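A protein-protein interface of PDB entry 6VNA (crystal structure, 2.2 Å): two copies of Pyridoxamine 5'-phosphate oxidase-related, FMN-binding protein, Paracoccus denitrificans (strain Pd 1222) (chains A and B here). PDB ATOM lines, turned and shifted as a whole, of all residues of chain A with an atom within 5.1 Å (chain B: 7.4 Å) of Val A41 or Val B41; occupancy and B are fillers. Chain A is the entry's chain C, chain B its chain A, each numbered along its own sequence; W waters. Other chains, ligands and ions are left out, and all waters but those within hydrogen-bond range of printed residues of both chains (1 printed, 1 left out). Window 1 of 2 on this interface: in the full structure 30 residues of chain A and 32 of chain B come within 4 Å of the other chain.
Val A41 touches five residues of chain B.
Printed residues of chain B within 4 Å of Arg A43: Leu B77 and Arg B92.
Printed residues of chain A within 4 Å of Gly B30: Pro A39 and Val A41.
Of the printed residues of chain A, Thr B31 touches Pro A39.
Of chain A, only Ser A28, Gly A30, Val A41, Gly A75, Leu A77 and Ser A94 come within 4 Å of Val B41.
Leu B93 touches none of the printed residues of chain A.
Leu B139 touches none of the printed residues of chain A.
The nearest residue of chain B that does not touch Val A41 is Gly B75 (4.1 Å).
The nearest residue of chain A that does not touch Val B41 is Leu A76 (4.1 Å).
The side-chain hydroxyl (OG) of Ser A94 sits at hydrogen-bond distance from the backbone carbonyl oxygen (O) of Val B41 (2.6 Å).
The backbone NH (N) of Gly B75 sits close to the backbone carbonyl oxygen (O) of Pro A39, at 3.4 Å.
The side-chain hydroxyl of Ser B94 is in hydrogen-bond range of the backbone carbonyl oxygen of Val A41, at 2.6 Å.
The side-chain hydroxyl (OG) of Ser B28 sits at hydrogen-bond distance from the side-chain hydroxyl (OG) of Ser A28 (2.8 Å).
Of the 12 printed residues of chain A, 10 touch a printed residue of chain B.
Hydrophobic or aromatic side chains of chain A within 4 Å of the printed part of chain B: Pro A39, Val A41 and Leu A77.
Of the 23 printed residues of chain B, 13 touch a printed residue of chain A.
Hydrophobic or aromatic side chains of chain B that line the printed part of chain A: Pro B39, Leu B40, Val B41, Leu B77 and Leu B96.
Among the printed residues, 28 pairs touch across the chains.
Water W1 lies within hydrogen-bond range of O of Arg A43 and NH2 of Arg B92.
O of Gly A30 touches CG of Pro B39, 3.6 Å away.
Val B41 touches Gly A30.
Thr B31 touches Pro A39 (C to CG, 3.8 Å).
O of Pro A39 touches CD2 of Leu B96 (3.4 Å).
CG1 of Val A41 touches CG1 of Val B41, 3.96 Å away.
CD1 of Leu B77 touches O of Val A41, 3.7 Å away.
Leu B77 touches Thr A42 (CD2 to C, 3.6 Å).
Ser B94 touches Thr A42 (OG to CG2, 3.4 Å).
Arg A43 touches Leu B77 (N to CD2, 3.5 Å).
Ser B28 touches Leu A77 (OG to CD2, 3.7 Å).
The backbone NH of Gly B30 lies within hydrogen-bond range of the backbone carbonyl oxygen of Gly B75 (2.7 Å).
The backbone NH of Leu B40 lies within hydrogen-bond range of the backbone carbonyl oxygen of Thr B31 (2.6 Å).
The backbone carbonyl oxygen (O) of Ser B28 sits at hydrogen-bond distance from the backbone NH (N) of Leu B77, 3.0 Å away.
The backbone NH (N) of Leu A29 is in hydrogen-bond range of the backbone carbonyl oxygen (O) of Thr A42, 2.8 Å away.
ND1 of His B64 is in hydrogen-bond range of OG1 of Thr B42.
O of Ser B94 sits at hydrogen-bond distance from N of Leu B139 (2.7 Å).
Gly A30 touches Val B41, and with the chains exchanged Val A41 touches Gly B30.
Pro A39 touches Gly B75, and with the chains exchanged Gly A75 touches Pro B39.
Thr A42 touches Leu B77, and with the chains exchanged Leu A77 touches Thr B42.
Gly A75 touches Val B41, but with the chains exchanged Val A41 does not touch Gly B75 (4.1 Å).
Of the 28 pairs that touch across the chains among the printed residues, 22 have their exchanged pair printed and touching as well.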
ATOM      1  N   SER A  28       1.897  22.034 -15.348  1.00  0.00           N
ATOM      2  CA  SER A  28       2.667  21.913 -16.608  1.00  0.00           C
ATOM      3  C   SER A  28       3.485  23.196 -16.777  1.00  0.00           C
ATOM      4  O   SER A  28       2.870  24.284 -16.835  1.00  0.00           O
ATOM      5  CB  SER A  28       1.789  21.652 -17.798  1.00  0.00           C
ATOM      6  OG  SER A  28       0.994  20.497 -17.606  1.00  0.00           O
ATOM      7  N   LEU A  29       4.816  23.059 -16.786  1.00  0.00           N
ATOM      8  CA  LEU A  29       5.770  24.151 -17.070  1.00  0.00           C
ATOM      9  C   LEU A  29       6.060  24.130 -18.565  1.00  0.00           C
ATOM     10  O   LEU A  29       6.242  23.027 -19.100  1.00  0.00           O
ATOM     11  CB  LEU A  29       7.064  23.954 -16.280  1.00  0.00           C
ATOM     12  CG  LEU A  29       8.088  25.082 -16.400  1.00  0.00           C
ATOM     13  CD1 LEU A  29       7.524  26.381 -15.885  1.00  0.00           C
ATOM     14  CD2 LEU A  29       9.349  24.753 -15.636  1.00  0.00           C
ATOM     15  N   GLY A  30       6.031  25.312 -19.187  1.00  0.00           N
ATOM     16  CA  GLY A  30       6.506  25.554 -20.557  1.00  0.00           C
ATOM     17  C   GLY A  30       7.775  26.381 -20.529  1.00  0.00           C
ATOM     18  O   GLY A  30       7.770  27.510 -19.965  1.00  0.00           O
ATOM     19  N   PRO A  39       8.439  24.941 -27.718  1.00  0.00           N
ATOM     20  CA  PRO A  39       8.058  24.814 -26.313  1.00  0.00           C
ATOM     21  C   PRO A  39       8.222  23.364 -25.811  1.00  0.00           C
ATOM     22  O   PRO A  39       7.615  22.455 -26.356  1.00  0.00           O
ATOM     23  CB  PRO A  39       6.573  25.233 -26.277  1.00  0.00           C
ATOM     24  CG  PRO A  39       6.362  26.002 -27.554  1.00  0.00           C
ATOM     25  CD  PRO A  39       7.301  25.353 -28.546  1.00  0.00           C
ATOM     26  N   LEU A  40       9.119  23.185 -24.851  1.00  0.00           N
ATOM     27  CA  LEU A  40       9.243  21.976 -24.001  1.00  0.00           C
ATOM     28  C   LEU A  40       8.217  22.092 -22.858  1.00  0.00           C
ATOM     29  O   LEU A  40       8.248  23.131 -22.120  1.00  0.00           O
ATOM     30  CB  LEU A  40      10.682  21.907 -23.469  1.00  0.00           C
ATOM     31  CG  LEU A  40      10.929  20.809 -22.442  1.00  0.00           C
ATOM     32  CD1 LEU A  40      10.822  19.437 -23.097  1.00  0.00           C
ATOM     33  CD2 LEU A  40      12.265  20.998 -21.760  1.00  0.00           C
ATOM     34  N   VAL A  41       7.333  21.096 -22.723  1.00  0.00           N
ATOM     35  CA  VAL A  41       6.299  21.040 -21.643  1.00  0.00           C
ATOM     36  C   VAL A  41       6.571  19.822 -20.760  1.00  0.00           C
ATOM     37  O   VAL A  41       6.527  18.672 -21.266  1.00  0.00           O
ATOM     38  CB  VAL A  41       4.866  21.009 -22.206  1.00  0.00           C
ATOM     39  CG1 VAL A  41       3.840  21.128 -21.103  1.00  0.00           C
ATOM     40  CG2 VAL A  41       4.647  22.103 -23.222  1.00  0.00           C
ATOM     41  N   THR A  42       6.828  20.073 -19.481  1.00  0.00           N
ATOM     42  CA  THR A  42       7.105  19.045 -18.451  1.00  0.00           C
ATOM     43  C   THR A  42       6.259  19.338 -17.213  1.00  0.00           C
ATOM     44  O   THR A  42       5.759  20.454 -17.106  1.00  0.00           O
ATOM     45  CB  THR A  42       8.587  19.037 -18.078  1.00  0.00           C
ATOM     46  OG1 THR A  42       8.813  20.290 -17.432  1.00  0.00           O
ATOM     47  CG2 THR A  42       9.480  18.798 -19.275  1.00  0.00           C
ATOM     48  N   ARG A  43       6.095  18.334 -16.347  1.00  0.00           N
ATOM     49  CA  ARG A  43       5.392  18.436 -15.045  1.00  0.00           C
ATOM     50  C   ARG A  43       6.384  18.897 -13.968  1.00  0.00           C
ATOM     51  O   ARG A  43       7.524  18.410 -13.937  1.00  0.00           O
ATOM     52  CB  ARG A  43       4.758  17.097 -14.670  1.00  0.00           C
ATOM     53  CG  ARG A  43       3.945  17.160 -13.388  1.00  0.00           C
ATOM     54  CD  ARG A  43       3.128  15.918 -13.145  1.00  0.00           C
ATOM     55  NE  ARG A  43       1.981  15.847 -14.031  1.00  0.00           N
ATOM     56  CZ  ARG A  43       1.233  14.766 -14.233  1.00  0.00           C
ATOM     57  NH1 ARG A  43       1.509  13.643 -13.599  1.00  0.00           N
ATOM     58  NH2 ARG A  43       0.215  14.808 -15.077  1.00  0.00           N
ATOM     59  N   GLY A  75       5.925  29.510 -19.374  1.00  0.00           N
ATOM     60  CA  GLY A  75       4.459  29.344 -19.266  1.00  0.00           C
ATOM     61  C   GLY A  75       4.114  28.334 -18.174  1.00  0.00           C
ATOM     62  O   GLY A  75       4.939  27.418 -17.935  1.00  0.00           O
ATOM     63  N   LEU A  76       2.965  28.486 -17.519  1.00  0.00           N
ATOM     64  CA  LEU A  76       2.427  27.524 -16.528  1.00  0.00           C
ATOM     65  C   LEU A  76       0.973  27.202 -16.883  1.00  0.00           C
ATOM     66  O   LEU A  76       0.259  28.095 -17.346  1.00  0.00           O
ATOM     67  CB  LEU A  76       2.506  28.136 -15.129  1.00  0.00           C
ATOM     68  CG  LEU A  76       3.892  28.282 -14.503  1.00  0.00           C
ATOM     69  CD1 LEU A  76       3.770  29.014 -13.176  1.00  0.00           C
ATOM     70  CD2 LEU A  76       4.561  26.938 -14.287  1.00  0.00           C
ATOM     71  N   LEU A  77       0.554  25.958 -16.677  1.00  0.00           N
ATOM     72  CA  LEU A  77      -0.877  25.573 -16.733  1.00  0.00           C
ATOM     73  C   LEU A  77      -1.216  24.952 -15.379  1.00  0.00           C
ATOM     74  O   LEU A  77      -0.486  24.039 -14.934  1.00  0.00           O
ATOM     75  CB  LEU A  77      -1.114  24.590 -17.883  1.00  0.00           C
ATOM     76  CG  LEU A  77      -2.492  23.934 -17.918  1.00  0.00           C
ATOM     77  CD1 LEU A  77      -3.577  24.969 -18.129  1.00  0.00           C
ATOM     78  CD2 LEU A  77      -2.580  22.864 -18.999  1.00  0.00           C
ATOM     79  N   SER A  94      -3.750  29.528 -17.464  1.00  0.00           N
ATOM     80  CA  SER A  94      -2.471  29.668 -18.190  1.00  0.00           C
ATOM     81  C   SER A  94      -1.795  30.974 -17.743  1.00  0.00           C
ATOM     82  O   SER A  94      -2.468  31.988 -17.683  1.00  0.00           O
ATOM     83  CB  SER A  94      -2.715  29.651 -19.665  1.00  0.00           C
ATOM     84  OG  SER A  94      -3.322  28.434 -20.054  1.00  0.00           O
ATOM     85  N   ALA B  27      -4.069  16.336 -23.285  1.00  0.00           N
ATOM     86  CA  ALA B  27      -2.660  16.709 -23.083  1.00  0.00           C
ATOM     87  C   ALA B  27      -2.532  18.172 -22.657  1.00  0.00           C
ATOM     88  O   ALA B  27      -3.520  18.945 -22.793  1.00  0.00           O
ATOM     89  CB  ALA B  27      -1.895  16.469 -24.358  1.00  0.00           C
ATOM     90  N   SER B  28      -1.336  18.533 -22.199  1.00  0.00           N
ATOM     91  CA  SER B  28      -0.892  19.938 -22.104  1.00  0.00           C
ATOM     92  C   SER B  28      -0.204  20.300 -23.423  1.00  0.00           C
ATOM     93  O   SER B  28       0.774  19.621 -23.774  1.00  0.00           O
ATOM     94  CB  SER B  28       0.024  20.145 -20.933  1.00  0.00           C
ATOM     95  OG  SER B  28      -0.616  19.804 -19.734  1.00  0.00           O
ATOM     96  N   LEU B  29      -0.696  21.306 -24.136  1.00  0.00           N
ATOM     97  CA  LEU B  29      -0.061  21.766 -25.408  1.00  0.00           C
ATOM     98  C   LEU B  29       0.716  23.054 -25.124  1.00  0.00           C
ATOM     99  O   LEU B  29       0.160  23.979 -24.470  1.00  0.00           O
ATOM    100  CB  LEU B  29      -1.138  21.976 -26.467  1.00  0.00           C
ATOM    101  CG  LEU B  29      -0.700  22.725 -27.727  1.00  0.00           C
ATOM    102  CD1 LEU B  29       0.151  21.844 -28.640  1.00  0.00           C
ATOM    103  CD2 LEU B  29      -1.923  23.234 -28.465  1.00  0.00           C
ATOM    104  N   GLY B  30       1.982  23.062 -25.505  1.00  0.00           N
ATOM    105  CA  GLY B  30       2.807  24.277 -25.554  1.00  0.00           C
ATOM    106  C   GLY B  30       2.766  24.933 -26.929  1.00  0.00           C
ATOM    107  O   GLY B  30       3.061  24.245 -27.955  1.00  0.00           O
ATOM    108  N   THR B  31       2.429  26.219 -26.963  1.00  0.00           N
ATOM    109  CA  THR B  31       2.584  27.083 -28.164  1.00  0.00           C
ATOM    110  C   THR B  31       3.374  28.355 -27.829  1.00  0.00           C
ATOM    111  O   THR B  31       3.533  28.714 -26.626  1.00  0.00           O
ATOM    112  CB  THR B  31       1.232  27.396 -28.797  1.00  0.00           C
ATOM    113  OG1 THR B  31       0.366  28.044 -27.860  1.00  0.00           O
ATOM    114  CG2 THR B  31       0.600  26.142 -29.367  1.00  0.00           C
ATOM    115  N   VAL B  38       6.813  33.871 -25.293  1.00  0.00           N
ATOM    116  CA  VAL B  38       6.696  33.052 -24.046  1.00  0.00           C
ATOM    117  C   VAL B  38       5.814  31.844 -24.354  1.00  0.00           C
ATOM    118  O   VAL B  38       4.819  31.984 -25.058  1.00  0.00           O
ATOM    119  CB  VAL B  38       6.084  33.857 -22.876  1.00  0.00           C
ATOM    120  CG1 VAL B  38       5.888  33.000 -21.631  1.00  0.00           C
ATOM    121  CG2 VAL B  38       6.903  35.082 -22.533  1.00  0.00           C
ATOM    122  N   PRO B  39       6.128  30.630 -23.832  1.00  0.00           N
ATOM    123  CA  PRO B  39       5.282  29.451 -24.069  1.00  0.00           C
ATOM    124  C   PRO B  39       3.899  29.634 -23.433  1.00  0.00           C
ATOM    125  O   PRO B  39       3.833  29.964 -22.265  1.00  0.00           O
ATOM    126  CB  PRO B  39       6.045  28.297 -23.403  1.00  0.00           C
ATOM    127  CG  PRO B  39       7.473  28.814 -23.273  1.00  0.00           C
ATOM    128  CD  PRO B  39       7.333  30.307 -23.046  1.00  0.00           C
ATOM    129  N   LEU B  40       2.836  29.505 -24.229  1.00  0.00           N
ATOM    130  CA  LEU B  40       1.439  29.379 -23.735  1.00  0.00           C
ATOM    131  C   LEU B  40       1.099  27.887 -23.528  1.00  0.00           C
ATOM    132  O   LEU B  40       1.171  27.113 -24.518  1.00  0.00           O
ATOM    133  CB  LEU B  40       0.500  29.987 -24.775  1.00  0.00           C
ATOM    134  CG  LEU B  40      -0.982  29.884 -24.430  1.00  0.00           C
ATOM    135  CD1 LEU B  40      -1.282  30.628 -23.129  1.00  0.00           C
ATOM    136  CD2 LEU B  40      -1.839  30.416 -25.561  1.00  0.00           C
ATOM    137  N   VAL B  41       0.765  27.486 -22.297  1.00  0.00           N
ATOM    138  CA  VAL B  41       0.460  26.066 -21.942  1.00  0.00           C
ATOM    139  C   VAL B  41      -1.037  25.958 -21.691  1.00  0.00           C
ATOM    140  O   VAL B  41      -1.523  26.632 -20.743  1.00  0.00           O
ATOM    141  CB  VAL B  41       1.292  25.591 -20.744  1.00  0.00           C
ATOM    142  CG1 VAL B  41       1.249  24.080 -20.620  1.00  0.00           C
ATOM    143  CG2 VAL B  41       2.736  26.074 -20.841  1.00  0.00           C
ATOM    144  N   THR B  42      -1.732  25.204 -22.553  1.00  0.00           N
ATOM    145  CA  THR B  42      -3.202  25.009 -22.523  1.00  0.00           C
ATOM    146  C   THR B  42      -3.525  23.506 -22.563  1.00  0.00           C
ATOM    147  O   THR B  42      -2.741  22.718 -23.099  1.00  0.00           O
ATOM    148  CB  THR B  42      -3.907  25.725 -23.680  1.00  0.00           C
ATOM    149  OG1 THR B  42      -3.432  25.172 -24.908  1.00  0.00           O
ATOM    150  CG2 THR B  42      -3.689  27.221 -23.706  1.00  0.00           C
ATOM    151  N   ARG B  43      -4.679  23.133 -22.027  1.00  0.00           N
ATOM    152  CA  ARG B  43      -5.158  21.734 -21.998  1.00  0.00           C
ATOM    153  C   ARG B  43      -5.980  21.487 -23.257  1.00  0.00           C
ATOM    154  O   ARG B  43      -6.872  22.294 -23.516  1.00  0.00           O
ATOM    155  CB  ARG B  43      -6.006  21.452 -20.754  1.00  0.00           C
ATOM    156  CG  ARG B  43      -6.480  20.010 -20.697  1.00  0.00           C
ATOM    157  CD  ARG B  43      -7.188  19.724 -19.407  1.00  0.00           C
ATOM    158  NE  ARG B  43      -6.265  19.426 -18.331  1.00  0.00           N
ATOM    159  CZ  ARG B  43      -6.612  19.322 -17.051  1.00  0.00           C
ATOM    160  NH1 ARG B  43      -7.870  19.504 -16.685  1.00  0.00           N
ATOM    161  NH2 ARG B  43      -5.697  19.025 -16.140  1.00  0.00           N
ATOM    162  N   HIS B  64      -4.388  29.206 -28.599  1.00  0.00           N
ATOM    163  CA  HIS B  64      -3.383  28.170 -28.955  1.00  0.00           C
ATOM    164  C   HIS B  64      -3.475  27.861 -30.454  1.00  0.00           C
ATOM    165  O   HIS B  64      -2.434  27.565 -31.056  1.00  0.00           O
ATOM    166  CB  HIS B  64      -3.488  26.909 -28.050  1.00  0.00           C
ATOM    167  CG  HIS B  64      -4.846  26.309 -27.898  1.00  0.00           C
ATOM    168  ND1 HIS B  64      -5.435  26.125 -26.667  1.00  0.00           N
ATOM    169  CD2 HIS B  64      -5.728  25.835 -28.807  1.00  0.00           C
ATOM    170  CE1 HIS B  64      -6.633  25.597 -26.823  1.00  0.00           C
ATOM    171  NE2 HIS B  64      -6.837  25.405 -28.127  1.00  0.00           N
ATOM    172  N   ALA B  74       5.379  23.330 -31.551  1.00  0.00           N
ATOM    173  CA  ALA B  74       4.389  22.794 -30.584  1.00  0.00           C
ATOM    174  C   ALA B  74       5.066  21.792 -29.659  1.00  0.00           C
ATOM    175  O   ALA B  74       5.795  20.922 -30.169  1.00  0.00           O
ATOM    176  CB  ALA B  74       3.229  22.152 -31.313  1.00  0.00           C
ATOM    177  N   GLY B  75       4.852  21.958 -28.353  1.00  0.00           N
ATOM    178  CA  GLY B  75       5.161  20.965 -27.301  1.00  0.00           C
ATOM    179  C   GLY B  75       3.920  20.226 -26.824  1.00  0.00           C
ATOM    180  O   GLY B  75       2.817  20.831 -26.791  1.00  0.00           O
ATOM    181  N   LEU B  76       4.062  18.946 -26.497  1.00  0.00           N
ATOM    182  CA  LEU B  76       2.999  18.161 -25.800  1.00  0.00           C
ATOM    183  C   LEU B  76       3.613  17.505 -24.569  1.00  0.00           C
ATOM    184  O   LEU B  76       4.740  16.945 -24.705  1.00  0.00           O
ATOM    185  CB  LEU B  76       2.434  17.065 -26.707  1.00  0.00           C
ATOM    186  CG  LEU B  76       1.698  17.513 -27.952  1.00  0.00           C
ATOM    187  CD1 LEU B  76       1.481  16.335 -28.895  1.00  0.00           C
ATOM    188  CD2 LEU B  76       0.375  18.151 -27.592  1.00  0.00           C
ATOM    189  N   LEU B  77       2.910  17.603 -23.432  1.00  0.00           N
ATOM    190  CA  LEU B  77       3.034  16.701 -22.262  1.00  0.00           C
ATOM    191  C   LEU B  77       1.858  15.720 -22.255  1.00  0.00           C
ATOM    192  O   LEU B  77       0.684  16.157 -22.267  1.00  0.00           O
ATOM    193  CB  LEU B  77       3.016  17.503 -20.960  1.00  0.00           C
ATOM    194  CG  LEU B  77       3.310  16.678 -19.705  1.00  0.00           C
ATOM    195  CD1 LEU B  77       4.594  15.863 -19.882  1.00  0.00           C
ATOM    196  CD2 LEU B  77       3.433  17.585 -18.485  1.00  0.00           C
ATOM    197  N   ILE B  78       2.162  14.437 -22.199  1.00  0.00           N
ATOM    198  CA  ILE B  78       1.145  13.346 -22.152  1.00  0.00           C
ATOM    199  C   ILE B  78       1.412  12.536 -20.882  1.00  0.00           C
ATOM    200  O   ILE B  78       2.498  11.987 -20.726  1.00  0.00           O
ATOM    201  CB  ILE B  78       1.222  12.540 -23.458  1.00  0.00           C
ATOM    202  CG1 ILE B  78       0.954  13.459 -24.649  1.00  0.00           C
ATOM    203  CG2 ILE B  78       0.291  11.340 -23.432  1.00  0.00           C
ATOM    204  CD1 ILE B  78       1.375  12.880 -25.967  1.00  0.00           C
ATOM    205  N   ARG B  92       5.075  10.026 -17.783  1.00  0.00           N
ATOM    206  CA  ARG B  92       4.735  11.189 -18.637  1.00  0.00           C
ATOM    207  C   ARG B  92       5.775  11.399 -19.725  1.00  0.00           C
ATOM    208  O   ARG B  92       7.000  11.232 -19.486  1.00  0.00           O
ATOM    209  CB  ARG B  92       4.647  12.450 -17.786  1.00  0.00           C
ATOM    210  CG  ARG B  92       5.931  12.724 -17.026  1.00  0.00           C
ATOM    211  CD  ARG B  92       5.543  13.200 -15.651  1.00  0.00           C
ATOM    212  NE  ARG B  92       6.649  13.792 -14.923  1.00  0.00           N
ATOM    213  CZ  ARG B  92       7.112  13.386 -13.758  1.00  0.00           C
ATOM    214  NH1 ARG B  92       6.612  12.320 -13.141  1.00  0.00           N
ATOM    215  NH2 ARG B  92       8.112  14.056 -13.223  1.00  0.00           N
ATOM    216  N   LEU B  93       5.277  11.768 -20.890  1.00  0.00           N
ATOM    217  CA  LEU B  93       6.075  11.899 -22.129  1.00  0.00           C
ATOM    218  C   LEU B  93       5.984  13.356 -22.592  1.00  0.00           C
ATOM    219  O   LEU B  93       4.824  13.864 -22.686  1.00  0.00           O
ATOM    220  CB  LEU B  93       5.480  10.932 -23.158  1.00  0.00           C
ATOM    221  CG  LEU B  93       6.112  11.046 -24.536  1.00  0.00           C
ATOM    222  CD1 LEU B  93       7.583  10.661 -24.461  1.00  0.00           C
ATOM    223  CD2 LEU B  93       5.344  10.199 -25.548  1.00  0.00           C
ATOM    224  N   SER B  94       7.136  14.005 -22.788  1.00  0.00           N
ATOM    225  CA  SER B  94       7.277  15.362 -23.386  1.00  0.00           C
ATOM    226  C   SER B  94       7.637  15.183 -24.850  1.00  0.00           C
ATOM    227  O   SER B  94       8.676  14.563 -25.115  1.00  0.00           O
ATOM    228  CB  SER B  94       8.351  16.193 -22.745  1.00  0.00           C
ATOM    229  OG  SER B  94       8.008  16.543 -21.422  1.00  0.00           O
ATOM    230  N   ILE B  95       6.844  15.738 -25.753  1.00  0.00           N
ATOM    231  CA  ILE B  95       7.186  15.732 -27.200  1.00  0.00           C
ATOM    232  C   ILE B  95       7.450  17.164 -27.660  1.00  0.00           C
ATOM    233  O   ILE B  95       6.718  18.047 -27.236  1.00  0.00           O
ATOM    234  CB  ILE B  95       6.060  15.057 -27.985  1.00  0.00           C
ATOM    235  CG1 ILE B  95       5.970  13.591 -27.576  1.00  0.00           C
ATOM    236  CG2 ILE B  95       6.252  15.238 -29.482  1.00  0.00           C
ATOM    237  CD1 ILE B  95       4.833  12.866 -28.228  1.00  0.00           C
ATOM    238  N   LEU B  96       8.504  17.340 -28.458  1.00  0.00           N
ATOM    239  CA  LEU B  96       8.785  18.539 -29.287  1.00  0.00           C
ATOM    240  C   LEU B  96       8.362  18.187 -30.716  1.00  0.00           C
ATOM    241  O   LEU B  96       8.812  17.159 -31.209  1.00  0.00           O
ATOM    242  CB  LEU B  96      10.274  18.893 -29.229  1.00  0.00           C
ATOM    243  CG  LEU B  96      10.875  19.265 -27.869  1.00  0.00           C
ATOM    244  CD1 LEU B  96      12.345  19.629 -28.010  1.00  0.00           C
ATOM    245  CD2 LEU B  96      10.138  20.409 -27.200  1.00  0.00           C
ATOM    246  N   LEU B 139      11.003  13.376 -24.489  1.00  0.00           N
ATOM    247  CA  LEU B 139      11.576  13.087 -23.149  1.00  0.00           C
ATOM    248  C   LEU B 139      10.610  12.159 -22.391  1.00  0.00           C
ATOM    249  O   LEU B 139       9.441  12.542 -22.187  1.00  0.00           O
ATOM    250  CB  LEU B 139      11.785  14.428 -22.439  1.00  0.00           C
ATOM    251  CG  LEU B 139      13.005  14.536 -21.531  1.00  0.00           C
ATOM    252  CD1 LEU B 139      14.238  13.911 -22.170  1.00  0.00           C
ATOM    253  CD2 LEU B 139      13.275  15.989 -21.172  1.00  0.00           C
HETATM  254  O   HOH W   1       9.547  16.854 -14.044  1.00  0.00           O
